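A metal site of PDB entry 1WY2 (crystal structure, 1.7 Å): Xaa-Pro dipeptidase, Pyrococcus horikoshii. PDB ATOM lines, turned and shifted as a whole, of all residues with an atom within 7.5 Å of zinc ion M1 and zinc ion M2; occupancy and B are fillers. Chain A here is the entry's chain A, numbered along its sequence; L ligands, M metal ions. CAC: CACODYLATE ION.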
ATOM      1  N   PHE A 181       3.932  -0.102  -9.452  1.00  0.00           N
ATOM      2  CA  PHE A 181       4.968  -0.341 -10.430  1.00  0.00           C
ATOM      3  C   PHE A 181       6.294  -0.475  -9.684  1.00  0.00           C
ATOM      4  O   PHE A 181       6.369  -0.165  -8.507  1.00  0.00           O
ATOM      5  CB  PHE A 181       5.019   0.825 -11.436  1.00  0.00           C
ATOM      6  CG  PHE A 181       5.153   2.175 -10.794  1.00  0.00           C
ATOM      7  CD1 PHE A 181       6.395   2.678 -10.453  1.00  0.00           C
ATOM      8  CD2 PHE A 181       4.014   2.941 -10.523  1.00  0.00           C
ATOM      9  CE1 PHE A 181       6.525   3.931  -9.858  1.00  0.00           C
ATOM     10  CE2 PHE A 181       4.133   4.203  -9.925  1.00  0.00           C
ATOM     11  CZ  PHE A 181       5.377   4.700  -9.592  1.00  0.00           C
ATOM     12  N   ILE A 184      11.119   3.283  -7.935  1.00  0.00           N
ATOM     13  CA  ILE A 184      12.312   3.962  -8.395  1.00  0.00           C
ATOM     14  C   ILE A 184      12.963   4.730  -7.249  1.00  0.00           C
ATOM     15  O   ILE A 184      12.343   5.601  -6.651  1.00  0.00           O
ATOM     16  CB  ILE A 184      11.967   4.951  -9.533  1.00  0.00           C
ATOM     17  CG1 ILE A 184      11.617   4.181 -10.801  1.00  0.00           C
ATOM     18  CG2 ILE A 184      13.141   5.914  -9.781  1.00  0.00           C
ATOM     19  CD1 ILE A 184      10.940   5.012 -11.867  1.00  0.00           C
ATOM     20  N   HIS A 195      13.635   6.282 -15.528  1.00  0.00           N
ATOM     21  CA  HIS A 195      13.106   5.039 -14.979  1.00  0.00           C
ATOM     22  C   HIS A 195      14.171   4.210 -14.262  1.00  0.00           C
ATOM     23  O   HIS A 195      14.239   2.993 -14.427  1.00  0.00           O
ATOM     24  CB  HIS A 195      12.463   4.202 -16.089  1.00  0.00           C
ATOM     25  CG  HIS A 195      11.151   4.750 -16.576  1.00  0.00           C
ATOM     26  ND1 HIS A 195      10.535   4.304 -17.718  1.00  0.00           N
ATOM     27  CD2 HIS A 195      10.344   5.713 -16.056  1.00  0.00           C
ATOM     28  CE1 HIS A 195       9.397   4.957 -17.891  1.00  0.00           C
ATOM     29  NE2 HIS A 195       9.262   5.823 -16.889  1.00  0.00           N
ATOM     30  N   ILE A 211      12.657   9.697  -5.998  1.00  0.00           N
ATOM     31  CA  ILE A 211      11.809   8.660  -5.407  1.00  0.00           C
ATOM     32  C   ILE A 211      10.467   8.664  -6.144  1.00  0.00           C
ATOM     33  O   ILE A 211       9.666   9.570  -5.969  1.00  0.00           O
ATOM     34  CB  ILE A 211      11.551   8.964  -3.913  1.00  0.00           C
ATOM     35  CG1 ILE A 211      12.896   9.141  -3.186  1.00  0.00           C
ATOM     36  CG2 ILE A 211      10.756   7.828  -3.278  1.00  0.00           C
ATOM     37  CD1 ILE A 211      12.773   9.834  -1.841  1.00  0.00           C
ATOM     38  N   ASP A 212      10.242   7.652  -6.978  1.00  0.00           N
ATOM     39  CA  ASP A 212       9.012   7.536  -7.763  1.00  0.00           C
ATOM     40  C   ASP A 212       8.381   6.197  -7.390  1.00  0.00           C
ATOM     41  O   ASP A 212       8.959   5.133  -7.634  1.00  0.00           O
ATOM     42  CB  ASP A 212       9.349   7.584  -9.260  1.00  0.00           C
ATOM     43  CG  ASP A 212       8.132   7.800 -10.141  1.00  0.00           C
ATOM     44  OD1 ASP A 212       6.994   7.520  -9.710  1.00  0.00           O
ATOM     45  OD2 ASP A 212       8.320   8.235 -11.297  1.00  0.00           O
ATOM     46  N   LEU A 213       7.197   6.235  -6.803  1.00  0.00           N
ATOM     47  CA  LEU A 213       6.524   5.029  -6.383  1.00  0.00           C
ATOM     48  C   LEU A 213       5.022   5.194  -6.419  1.00  0.00           C
ATOM     49  O   LEU A 213       4.507   6.288  -6.673  1.00  0.00           O
ATOM     50  CB  LEU A 213       6.985   4.657  -4.958  1.00  0.00           C
ATOM     51  CG  LEU A 213       6.762   5.691  -3.847  1.00  0.00           C
ATOM     52  CD1 LEU A 213       5.331   5.612  -3.338  1.00  0.00           C
ATOM     53  CD2 LEU A 213       7.737   5.423  -2.690  1.00  0.00           C
ATOM     54  N   GLY A 214       4.300   4.098  -6.186  1.00  0.00           N
ATOM     55  CA  GLY A 214       2.856   4.177  -6.197  1.00  0.00           C
ATOM     56  C   GLY A 214       2.266   2.918  -5.581  1.00  0.00           C
ATOM     57  O   GLY A 214       2.942   1.890  -5.500  1.00  0.00           O
ATOM     58  N   SER A 222      -1.963   4.827  -7.728  1.00  0.00           N
ATOM     59  CA  SER A 222      -1.493   6.130  -7.280  1.00  0.00           C
ATOM     60  C   SER A 222      -0.088   6.273  -7.864  1.00  0.00           C
ATOM     61  O   SER A 222       0.549   5.283  -8.228  1.00  0.00           O
ATOM     62  CB  SER A 222      -1.458   6.216  -5.754  1.00  0.00           C
ATOM     63  OG  SER A 222      -0.691   5.164  -5.196  1.00  0.00           O
ATOM     64  N   ASP A 223       0.414   7.496  -7.948  1.00  0.00           N
ATOM     65  CA  ASP A 223       1.722   7.732  -8.547  1.00  0.00           C
ATOM     66  C   ASP A 223       2.276   9.035  -7.989  1.00  0.00           C
ATOM     67  O   ASP A 223       1.612  10.067  -8.045  1.00  0.00           O
ATOM     68  CB  ASP A 223       1.542   7.821 -10.073  1.00  0.00           C
ATOM     69  CG  ASP A 223       2.836   7.686 -10.836  1.00  0.00           C
ATOM     70  OD1 ASP A 223       3.927   7.647 -10.210  1.00  0.00           O
ATOM     71  OD2 ASP A 223       2.752   7.619 -12.080  1.00  0.00           O
ATOM     72  N   ILE A 224       3.496   8.990  -7.457  1.00  0.00           N
ATOM     73  CA  ILE A 224       4.112  10.173  -6.887  1.00  0.00           C
ATOM     74  C   ILE A 224       5.629  10.148  -7.015  1.00  0.00           C
ATOM     75  O   ILE A 224       6.236   9.089  -6.969  1.00  0.00           O
ATOM     76  CB  ILE A 224       3.732  10.305  -5.387  1.00  0.00           C
ATOM     77  CG1 ILE A 224       4.268  11.611  -4.797  1.00  0.00           C
ATOM     78  CG2 ILE A 224       4.298   9.123  -4.600  1.00  0.00           C
ATOM     79  CD1 ILE A 224       3.912  11.822  -3.319  1.00  0.00           C
ATOM     80  N   THR A 225       6.237  11.321  -7.208  1.00  0.00           N
ATOM     81  CA  THR A 225       7.691  11.429  -7.295  1.00  0.00           C
ATOM     82  C   THR A 225       8.153  12.638  -6.514  1.00  0.00           C
ATOM     83  O   THR A 225       7.621  13.735  -6.675  1.00  0.00           O
ATOM     84  CB  THR A 225       8.227  11.616  -8.742  1.00  0.00           C
ATOM     85  OG1 THR A 225       7.834  10.522  -9.569  1.00  0.00           O
ATOM     86  CG2 THR A 225       9.756  11.686  -8.732  1.00  0.00           C
ATOM     87  N   LEU A 285       4.621  15.318 -20.001  1.00  0.00           N
ATOM     88  CA  LEU A 285       4.373  15.923 -18.706  1.00  0.00           C
ATOM     89  C   LEU A 285       3.633  14.979 -17.763  1.00  0.00           C
ATOM     90  O   LEU A 285       3.808  15.047 -16.544  1.00  0.00           O
ATOM     91  CB  LEU A 285       3.547  17.202 -18.864  1.00  0.00           C
ATOM     92  CG  LEU A 285       3.181  17.912 -17.563  1.00  0.00           C
ATOM     93  CD1 LEU A 285       4.449  18.337 -16.827  1.00  0.00           C
ATOM     94  CD2 LEU A 285       2.301  19.115 -17.859  1.00  0.00           C
ATOM     95  N   GLY A 286       2.796  14.106 -18.310  1.00  0.00           N
ATOM     96  CA  GLY A 286       2.061  13.199 -17.452  1.00  0.00           C
ATOM     97  C   GLY A 286       1.197  12.185 -18.146  1.00  0.00           C
ATOM     98  O   GLY A 286       1.215  12.063 -19.373  1.00  0.00           O
ATOM     99  N   HIS A 287       0.421  11.452 -17.355  1.00  0.00           N
ATOM    100  CA  HIS A 287      -0.443  10.398 -17.874  1.00  0.00           C
ATOM    101  C   HIS A 287      -1.648  10.212 -16.968  1.00  0.00           C
ATOM    102  O   HIS A 287      -1.610  10.577 -15.790  1.00  0.00           O
ATOM    103  CB  HIS A 287       0.350   9.083 -17.938  1.00  0.00           C
ATOM    104  CG  HIS A 287       0.980   8.703 -16.632  1.00  0.00           C
ATOM    105  ND1 HIS A 287       0.288   8.043 -15.630  1.00  0.00           N
ATOM    106  CD2 HIS A 287       2.209   8.953 -16.135  1.00  0.00           C
ATOM    107  CE1 HIS A 287       1.075   7.906 -14.580  1.00  0.00           C
ATOM    108  NE2 HIS A 287       2.248   8.456 -14.860  1.00  0.00           N
ATOM    109  N   GLY A 288      -2.723   9.663 -17.516  1.00  0.00           N
ATOM    110  CA  GLY A 288      -3.894   9.419 -16.710  1.00  0.00           C
ATOM    111  C   GLY A 288      -3.611   8.268 -15.766  1.00  0.00           C
ATOM    112  O   GLY A 288      -2.690   7.483 -16.001  1.00  0.00           O
ATOM    113  N   VAL A 289      -4.383   8.185 -14.681  1.00  0.00           N
ATOM    114  CA  VAL A 289      -4.223   7.138 -13.681  1.00  0.00           C
ATOM    115  C   VAL A 289      -5.603   6.604 -13.298  1.00  0.00           C
ATOM    116  O   VAL A 289      -6.565   7.369 -13.174  1.00  0.00           O
ATOM    117  CB  VAL A 289      -3.549   7.698 -12.401  1.00  0.00           C
ATOM    118  CG1 VAL A 289      -3.486   6.606 -11.338  1.00  0.00           C
ATOM    119  CG2 VAL A 289      -2.146   8.203 -12.721  1.00  0.00           C
ATOM    120  N   VAL A 293      -1.813   2.212 -14.044  1.00  0.00           N
ATOM    121  CA  VAL A 293      -1.008   3.373 -13.677  1.00  0.00           C
ATOM    122  C   VAL A 293      -0.804   4.316 -14.860  1.00  0.00           C
ATOM    123  O   VAL A 293      -0.650   5.523 -14.674  1.00  0.00           O
ATOM    124  CB  VAL A 293       0.354   2.948 -13.072  1.00  0.00           C
ATOM    125  CG1 VAL A 293       1.293   2.484 -14.149  1.00  0.00           C
ATOM    126  CG2 VAL A 293       0.953   4.111 -12.281  1.00  0.00           C
ATOM    127  N   HIS A 294      -0.813   3.755 -16.072  1.00  0.00           N
ATOM    128  CA  HIS A 294      -0.683   4.551 -17.290  1.00  0.00           C
ATOM    129  C   HIS A 294      -1.951   4.382 -18.137  1.00  0.00           C
ATOM    130  O   HIS A 294      -2.163   3.316 -18.720  1.00  0.00           O
ATOM    131  CB  HIS A 294       0.511   4.093 -18.137  1.00  0.00           C
ATOM    132  CG  HIS A 294       1.839   4.402 -17.528  1.00  0.00           C
ATOM    133  ND1 HIS A 294       2.695   3.415 -17.087  1.00  0.00           N
ATOM    134  CD2 HIS A 294       2.471   5.574 -17.304  1.00  0.00           C
ATOM    135  CE1 HIS A 294       3.799   3.972 -16.623  1.00  0.00           C
ATOM    136  NE2 HIS A 294       3.683   5.280 -16.745  1.00  0.00           N
ATOM    137  N   THR A 314      -1.362  12.745 -13.930  1.00  0.00           N
ATOM    138  CA  THR A 314      -0.174  13.106 -13.174  1.00  0.00           C
ATOM    139  C   THR A 314       0.442  14.323 -13.866  1.00  0.00           C
ATOM    140  O   THR A 314       0.209  14.557 -15.046  1.00  0.00           O
ATOM    141  CB  THR A 314       0.882  11.984 -13.167  1.00  0.00           C
ATOM    142  OG1 THR A 314       1.306  11.716 -14.513  1.00  0.00           O
ATOM    143  CG2 THR A 314       0.329  10.718 -12.536  1.00  0.00           C
ATOM    144  N   ILE A 315       1.188  15.101 -13.096  1.00  0.00           N
ATOM    145  CA  ILE A 315       1.893  16.274 -13.596  1.00  0.00           C
ATOM    146  C   ILE A 315       3.298  15.991 -13.075  1.00  0.00           C
ATOM    147  O   ILE A 315       3.562  16.090 -11.874  1.00  0.00           O
ATOM    148  CB  ILE A 315       1.341  17.577 -12.960  1.00  0.00           C
ATOM    149  CG1 ILE A 315      -0.131  17.759 -13.345  1.00  0.00           C
ATOM    150  CG2 ILE A 315       2.154  18.774 -13.432  1.00  0.00           C
ATOM    151  CD1 ILE A 315      -0.367  17.905 -14.838  1.00  0.00           C
ATOM    152  N   GLU A 316       4.200  15.620 -13.978  1.00  0.00           N
ATOM    153  CA  GLU A 316       5.541  15.254 -13.542  1.00  0.00           C
ATOM    154  C   GLU A 316       6.698  15.684 -14.428  1.00  0.00           C
ATOM    155  O   GLU A 316       7.362  14.849 -15.050  1.00  0.00           O
ATOM    156  CB  GLU A 316       5.603  13.739 -13.347  1.00  0.00           C
ATOM    157  CG  GLU A 316       5.171  12.929 -14.575  1.00  0.00           C
ATOM    158  CD  GLU A 316       5.171  11.428 -14.308  1.00  0.00           C
ATOM    159  OE1 GLU A 316       6.185  10.912 -13.804  1.00  0.00           O
ATOM    160  OE2 GLU A 316       4.153  10.772 -14.618  1.00  0.00           O
ATOM    161  N   ARG A 328      12.865  15.163 -10.612  1.00  0.00           N
ATOM    162  CA  ARG A 328      11.484  14.985 -11.052  1.00  0.00           C
ATOM    163  C   ARG A 328      10.562  15.186  -9.854  1.00  0.00           C
ATOM    164  O   ARG A 328      10.854  14.716  -8.746  1.00  0.00           O
ATOM    165  CB  ARG A 328      11.231  13.597 -11.652  1.00  0.00           C
ATOM    166  CG  ARG A 328       9.753  13.405 -12.048  1.00  0.00           C
ATOM    167  CD  ARG A 328       9.498  12.198 -12.982  1.00  0.00           C
ATOM    168  NE  ARG A 328       9.776  10.897 -12.373  1.00  0.00           N
ATOM    169  CZ  ARG A 328      10.908  10.221 -12.521  1.00  0.00           C
ATOM    170  NH1 ARG A 328      11.879  10.709 -13.264  1.00  0.00           N
ATOM    171  NH2 ARG A 328      11.045   9.019 -11.957  1.00  0.00           N
ATOM    172  N   GLU A 330       6.464  14.826  -9.095  1.00  0.00           N
ATOM    173  CA  GLU A 330       5.209  14.335  -9.634  1.00  0.00           C
ATOM    174  C   GLU A 330       4.065  14.221  -8.648  1.00  0.00           C
ATOM    175  O   GLU A 330       4.254  13.740  -7.525  1.00  0.00           O
ATOM    176  CB  GLU A 330       5.451  12.957 -10.273  1.00  0.00           C
ATOM    177  CG  GLU A 330       4.176  12.146 -10.528  1.00  0.00           C
ATOM    178  CD  GLU A 330       4.445  10.782 -11.119  1.00  0.00           C
ATOM    179  OE1 GLU A 330       5.437  10.145 -10.713  1.00  0.00           O
ATOM    180  OE2 GLU A 330       3.643  10.336 -11.954  1.00  0.00           O
ATOM    181  N   ASP A 331       2.883  14.674  -9.071  1.00  0.00           N
ATOM    182  CA  ASP A 331       1.667  14.585  -8.259  1.00  0.00           C
ATOM    183  C   ASP A 331       0.597  13.914  -9.095  1.00  0.00           C
ATOM    184  O   ASP A 331       0.628  13.982 -10.321  1.00  0.00           O
ATOM    185  CB  ASP A 331       1.112  15.969  -7.888  1.00  0.00           C
ATOM    186  CG  ASP A 331       1.779  16.580  -6.682  1.00  0.00           C
ATOM    187  OD1 ASP A 331       1.994  15.866  -5.680  1.00  0.00           O
ATOM    188  OD2 ASP A 331       2.056  17.801  -6.730  1.00  0.00           O
ATOM    189  N   THR A 332      -0.347  13.247  -8.434  1.00  0.00           N
ATOM    190  CA  THR A 332      -1.487  12.666  -9.128  1.00  0.00           C
ATOM    191  C   THR A 332      -2.536  13.715  -8.786  1.00  0.00           C
ATOM    192  O   THR A 332      -2.663  14.094  -7.615  1.00  0.00           O
ATOM    193  CB  THR A 332      -1.920  11.312  -8.551  1.00  0.00           C
ATOM    194  OG1 THR A 332      -0.949  10.325  -8.883  1.00  0.00           O
ATOM    195  CG2 THR A 332      -3.279  10.888  -9.116  1.00  0.00           C
HETATM  196 AS   CAC L   1       5.808   6.416 -13.834  1.00  0.00          AS
HETATM  197  O1  CAC L   1       5.494   7.858 -13.087  1.00  0.00           O
HETATM  198  O2  CAC L   1       5.659   6.687 -15.436  1.00  0.00           O
HETATM  199  C1  CAC L   1       7.559   5.843 -13.526  1.00  0.00           C
HETATM  200  C2  CAC L   1       4.514   5.133 -13.405  1.00  0.00           C
HETATM  201 ZN    ZN M   1       3.747   8.892 -13.456  1.00  0.00          ZN
HETATM  202 ZN    ZN M   2       5.659   8.196 -11.059  1.00  0.00          ZN
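O of Asp 223 lies within hydrogen-bond range of OG1 of Thr 332, 2.7 Å away.
The side-chain hydroxyl (OG1) of Thr 225 sits close to the side-chain carboxylate (OD2) of Asp 212.
NH2 of Arg 328 lies within salt-bridge range of OD2 of Asp 212, at 2.9 Å.
The backbone carbonyl oxygen (O) of Asp 212 is in hydrogen-bond range of the backbone NH (N) of Ile 184 (2.9 Å).
The backbone carbonyl oxygen of His 287 is in hydrogen-bond range of the backbone NH of Thr 314 (2.9 Å).
The side-chain carboxylate of Glu 316 lies close to the side-chain hydroxyl of Thr 314, at 3.0 Å.
OE1 of Glu 316 is in salt-bridge range of NE of Arg 328 (3.9 Å).
OG1 of Thr 225 lies within hydrogen-bond range of NE of Arg 328 (3.4 Å).
Thr 314 touches zinc ion M1.
Five residues have an atom within 4 Å of zinc ion M1: Asp 223, His 287, Thr 314, Glu 316 and Glu 330.
Zinc ion M1 is bound by an oxygen (O1) of the ligand (2.1 Å), the side-chain carboxylate (OE2) of Glu 330 (2.1 Å), a ring nitrogen (NE2) of His 287 (2.1 Å), the side-chain carboxylate (OD2) of Asp 223 (2.1 Å) and the side-chain carboxylate (OE2) of Glu 316 (2.2 Å).
Merely in contact with zinc ion M2: Phe 181 and Thr 225.
Six residues have an atom within 4 Å of zinc ion M2: Phe 181, Asp 212, Asp 223, Thr 225, Glu 316 and Glu 330.
Along chain A the residues within 4 Å of zinc ion M2 span positions 181 to 330.
The nearest printed residue that does not touch zinc ion M2 is Ile 224 (4.2 Å).
OE1 of Glu 330 is bound to zinc ion M2, at 2.0 Å.
Zinc ion M2 is bound by OD1 of Asp 223, 2.0 Å away.
OD1 of Asp 212 is bound to zinc ion M2.
O1 of the ligand binds zinc ion M2 (2.1 Å).
Zinc ion M2 has four donor atoms within binding distance.
Slightly farther from zinc ion M2 lies the side-chain carboxylate (OD2) of Asp 212 (2.7 Å).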
